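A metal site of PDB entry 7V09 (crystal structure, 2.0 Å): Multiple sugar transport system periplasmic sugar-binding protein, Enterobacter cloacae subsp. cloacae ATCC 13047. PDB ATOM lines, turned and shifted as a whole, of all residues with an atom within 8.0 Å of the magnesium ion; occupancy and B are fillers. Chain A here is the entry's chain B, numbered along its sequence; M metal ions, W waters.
The backbone carbonyl oxygen of Glu 143 sits close to a ring nitrogen (NE2) of His 145 (3.2 Å).
The nearest printed residue that does not touch the magnesium ion is Val 264 (4.1 Å).
The magnesium ion is bound by O of Phe 263 (2.0 Å), OE2 of Glu 143 (2.0 Å), OE2 of Glu 346 (2.1 Å) and water W1 (2.1 Å). The magnesium ion has four donor atoms within binding distance.
Water W1 bridges the backbone NH (N) of Phe 263 and the side-chain carboxylate (OE1) of Glu 346.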
ATOM      1  N   VAL A 129     -29.572   6.074  16.643  1.00  0.00           N
ATOM      2  CA  VAL A 129     -29.841   5.657  15.272  1.00  0.00           C
ATOM      3  C   VAL A 129     -28.606   5.951  14.434  1.00  0.00           C
ATOM      4  O   VAL A 129     -28.212   7.116  14.279  1.00  0.00           O
ATOM      5  CB  VAL A 129     -31.071   6.352  14.696  1.00  0.00           C
ATOM      6  CG1 VAL A 129     -31.245   6.010  13.223  1.00  0.00           C
ATOM      7  CG2 VAL A 129     -32.324   5.978  15.487  1.00  0.00           C
ATOM      8  N   TYR A 131     -26.522   5.498  10.668  1.00  0.00           N
ATOM      9  CA  TYR A 131     -26.871   5.454   9.256  1.00  0.00           C
ATOM     10  C   TYR A 131     -25.618   5.553   8.397  1.00  0.00           C
ATOM     11  O   TYR A 131     -24.593   6.091   8.826  1.00  0.00           O
ATOM     12  CB  TYR A 131     -27.845   6.576   8.876  1.00  0.00           C
ATOM     13  CG  TYR A 131     -27.229   7.967   8.818  1.00  0.00           C
ATOM     14  CD1 TYR A 131     -27.078   8.735   9.972  1.00  0.00           C
ATOM     15  CD2 TYR A 131     -26.818   8.507   7.609  1.00  0.00           C
ATOM     16  CE1 TYR A 131     -26.530   9.993   9.912  1.00  0.00           C
ATOM     17  CE2 TYR A 131     -26.268   9.776   7.548  1.00  0.00           C
ATOM     18  CZ  TYR A 131     -26.114  10.512   8.696  1.00  0.00           C
ATOM     19  OH  TYR A 131     -25.565  11.770   8.636  1.00  0.00           O
ATOM     20  N   LYS A 133     -23.788   7.368   5.650  1.00  0.00           N
ATOM     21  CA  LYS A 133     -23.888   8.737   5.158  1.00  0.00           C
ATOM     22  C   LYS A 133     -23.997   8.789   3.643  1.00  0.00           C
ATOM     23  O   LYS A 133     -24.617   9.728   3.104  1.00  0.00           O
ATOM     24  CB  LYS A 133     -22.697   9.557   5.647  1.00  0.00           C
ATOM     25  CG  LYS A 133     -22.329   9.308   7.097  1.00  0.00           C
ATOM     26  CD  LYS A 133     -21.161  10.170   7.542  1.00  0.00           C
ATOM     27  CE  LYS A 133     -21.636  11.332   8.411  1.00  0.00           C
ATOM     28  NZ  LYS A 133     -20.490  12.139   8.915  1.00  0.00           N
ATOM     29  N   GLU A 143     -29.947  14.331   7.263  1.00  0.00           N
ATOM     30  CA  GLU A 143     -29.992  13.809   8.618  1.00  0.00           C
ATOM     31  C   GLU A 143     -31.254  14.300   9.302  1.00  0.00           C
ATOM     32  O   GLU A 143     -31.409  15.518   9.516  1.00  0.00           O
ATOM     33  CB  GLU A 143     -28.733  14.217   9.397  1.00  0.00           C
ATOM     34  CG  GLU A 143     -28.265  13.203  10.420  1.00  0.00           C
ATOM     35  CD  GLU A 143     -27.589  13.843  11.604  1.00  0.00           C
ATOM     36  OE1 GLU A 143     -28.181  14.769  12.213  1.00  0.00           O
ATOM     37  OE2 GLU A 143     -26.443  13.443  11.923  1.00  0.00           O
ATOM     38  N   PRO A 144     -32.182  13.413   9.648  1.00  0.00           N
ATOM     39  CA  PRO A 144     -33.477  13.863  10.178  1.00  0.00           C
ATOM     40  C   PRO A 144     -33.347  14.529  11.541  1.00  0.00           C
ATOM     41  O   PRO A 144     -32.436  14.236  12.317  1.00  0.00           O
ATOM     42  CB  PRO A 144     -34.301  12.571  10.269  1.00  0.00           C
ATOM     43  CG  PRO A 144     -33.282  11.472  10.337  1.00  0.00           C
ATOM     44  CD  PRO A 144     -32.080  11.945   9.578  1.00  0.00           C
ATOM     45  N   HIS A 145     -34.284  15.438  11.812  1.00  0.00           N
ATOM     46  CA  HIS A 145     -34.282  16.207  13.059  1.00  0.00           C
ATOM     47  C   HIS A 145     -35.400  15.831  14.012  1.00  0.00           C
ATOM     48  O   HIS A 145     -35.423  16.358  15.133  1.00  0.00           O
ATOM     49  CB  HIS A 145     -34.372  17.712  12.753  1.00  0.00           C
ATOM     50  CG  HIS A 145     -33.405  18.186  11.720  1.00  0.00           C
ATOM     51  ND1 HIS A 145     -33.675  19.241  10.872  1.00  0.00           N
ATOM     52  CD2 HIS A 145     -32.155  17.770  11.409  1.00  0.00           C
ATOM     53  CE1 HIS A 145     -32.637  19.441  10.081  1.00  0.00           C
ATOM     54  NE2 HIS A 145     -31.703  18.563  10.382  1.00  0.00           N
ATOM     55  N   LEU A 261     -19.923   6.628   8.676  1.00  0.00           N
ATOM     56  CA  LEU A 261     -20.780   6.397   9.835  1.00  0.00           C
ATOM     57  C   LEU A 261     -21.377   7.722  10.302  1.00  0.00           C
ATOM     58  O   LEU A 261     -20.645   8.629  10.691  1.00  0.00           O
ATOM     59  CB  LEU A 261     -20.003   5.730  10.964  1.00  0.00           C
ATOM     60  CG  LEU A 261     -20.857   5.236  12.139  1.00  0.00           C
ATOM     61  CD1 LEU A 261     -22.124   4.546  11.639  1.00  0.00           C
ATOM     62  CD2 LEU A 261     -20.059   4.296  13.037  1.00  0.00           C
ATOM     63  N   GLY A 262     -22.699   7.812  10.271  1.00  0.00           N
ATOM     64  CA  GLY A 262     -23.396   8.971  10.794  1.00  0.00           C
ATOM     65  C   GLY A 262     -24.238   8.628  11.998  1.00  0.00           C
ATOM     66  O   GLY A 262     -24.526   7.453  12.245  1.00  0.00           O
ATOM     67  N   PHE A 263     -24.641   9.635  12.766  1.00  0.00           N
ATOM     68  CA  PHE A 263     -25.375   9.411  14.001  1.00  0.00           C
ATOM     69  C   PHE A 263     -26.450  10.464  14.155  1.00  0.00           C
ATOM     70  O   PHE A 263     -26.166  11.665  14.056  1.00  0.00           O
ATOM     71  CB  PHE A 263     -24.423   9.430  15.205  1.00  0.00           C
ATOM     72  CG  PHE A 263     -25.101   9.252  16.531  1.00  0.00           C
ATOM     73  CD1 PHE A 263     -25.409   7.976  16.987  1.00  0.00           C
ATOM     74  CD2 PHE A 263     -25.415  10.340  17.330  1.00  0.00           C
ATOM     75  CE1 PHE A 263     -26.029   7.807  18.213  1.00  0.00           C
ATOM     76  CE2 PHE A 263     -26.035  10.170  18.542  1.00  0.00           C
ATOM     77  CZ  PHE A 263     -26.349   8.905  18.991  1.00  0.00           C
ATOM     78  N   VAL A 264     -27.690  10.029  14.403  1.00  0.00           N
ATOM     79  CA  VAL A 264     -28.821  10.929  14.583  1.00  0.00           C
ATOM     80  C   VAL A 264     -29.528  10.582  15.880  1.00  0.00           C
ATOM     81  O   VAL A 264     -29.695   9.405  16.232  1.00  0.00           O
ATOM     82  CB  VAL A 264     -29.786  10.861  13.374  1.00  0.00           C
ATOM     83  CG1 VAL A 264     -30.088   9.424  13.000  1.00  0.00           C
ATOM     84  CG2 VAL A 264     -31.071  11.613  13.666  1.00  0.00           C
ATOM     85  N   VAL A 265     -29.903  11.586  16.661  1.00  0.00           N
ATOM     86  CA  VAL A 265     -30.588  11.407  17.937  1.00  0.00           C
ATOM     87  C   VAL A 265     -32.108  11.561  17.841  1.00  0.00           C
ATOM     88  O   VAL A 265     -32.613  12.560  17.406  1.00  0.00           O
ATOM     89  CB  VAL A 265     -29.927  12.150  19.118  1.00  0.00           C
ATOM     90  CG1 VAL A 265     -28.751  12.970  18.673  1.00  0.00           C
ATOM     91  CG2 VAL A 265     -30.860  12.975  19.916  1.00  0.00           C
ATOM     92  N   LEU A 343     -16.961  12.147  14.768  1.00  0.00           N
ATOM     93  CA  LEU A 343     -18.034  11.349  15.353  1.00  0.00           C
ATOM     94  C   LEU A 343     -17.925  11.186  16.872  1.00  0.00           C
ATOM     95  O   LEU A 343     -18.938  11.402  17.563  1.00  0.00           O
ATOM     96  CB  LEU A 343     -18.090   9.989  14.657  1.00  0.00           C
ATOM     97  CG  LEU A 343     -19.270   9.087  15.055  1.00  0.00           C
ATOM     98  CD1 LEU A 343     -20.522   9.496  14.305  1.00  0.00           C
ATOM     99  CD2 LEU A 343     -18.932   7.632  14.806  1.00  0.00           C
ATOM    100  N   GLU A 346     -19.114  14.366  18.559  1.00  0.00           N
ATOM    101  CA  GLU A 346     -20.560  14.489  18.443  1.00  0.00           C
ATOM    102  C   GLU A 346     -21.255  13.524  19.399  1.00  0.00           C
ATOM    103  O   GLU A 346     -22.295  13.861  19.988  1.00  0.00           O
ATOM    104  CB  GLU A 346     -21.002  14.224  17.004  1.00  0.00           C
ATOM    105  CG  GLU A 346     -22.515  14.273  16.805  1.00  0.00           C
ATOM    106  CD  GLU A 346     -22.933  13.815  15.422  1.00  0.00           C
ATOM    107  OE1 GLU A 346     -22.049  13.489  14.608  1.00  0.00           O
ATOM    108  OE2 GLU A 346     -24.156  13.783  15.154  1.00  0.00           O
ATOM    109  N   LEU A 347     -20.698  12.327  19.579  1.00  0.00           N
ATOM    110  CA  LEU A 347     -21.248  11.383  20.534  1.00  0.00           C
ATOM    111  C   LEU A 347     -21.074  11.885  21.966  1.00  0.00           C
ATOM    112  O   LEU A 347     -21.998  11.791  22.781  1.00  0.00           O
ATOM    113  CB  LEU A 347     -20.584  10.019  20.365  1.00  0.00           C
ATOM    114  CG  LEU A 347     -20.940   9.264  19.077  1.00  0.00           C
ATOM    115  CD1 LEU A 347     -20.192   7.943  19.012  1.00  0.00           C
ATOM    116  CD2 LEU A 347     -22.438   9.042  18.993  1.00  0.00           C
ATOM    117  N   GLN A 350     -23.568  14.635  22.947  1.00  0.00           N
ATOM    118  CA  GLN A 350     -24.931  14.238  23.265  1.00  0.00           C
ATOM    119  C   GLN A 350     -25.101  13.796  24.710  1.00  0.00           C
ATOM    120  O   GLN A 350     -26.160  13.270  25.066  1.00  0.00           O
ATOM    121  CB  GLN A 350     -25.379  13.103  22.330  1.00  0.00           C
ATOM    122  CG  GLN A 350     -25.615  13.548  20.894  1.00  0.00           C
ATOM    123  CD  GLN A 350     -26.333  14.879  20.802  1.00  0.00           C
ATOM    124  OE1 GLN A 350     -27.407  15.059  21.382  1.00  0.00           O
ATOM    125  NE2 GLN A 350     -25.748  15.817  20.067  1.00  0.00           N
HETATM  126 MG    MG M   1     -25.791  13.615  13.810  1.00  0.00          MG
HETATM  127  O   HOH W   1     -24.283  12.555  12.756  1.00  0.00           O
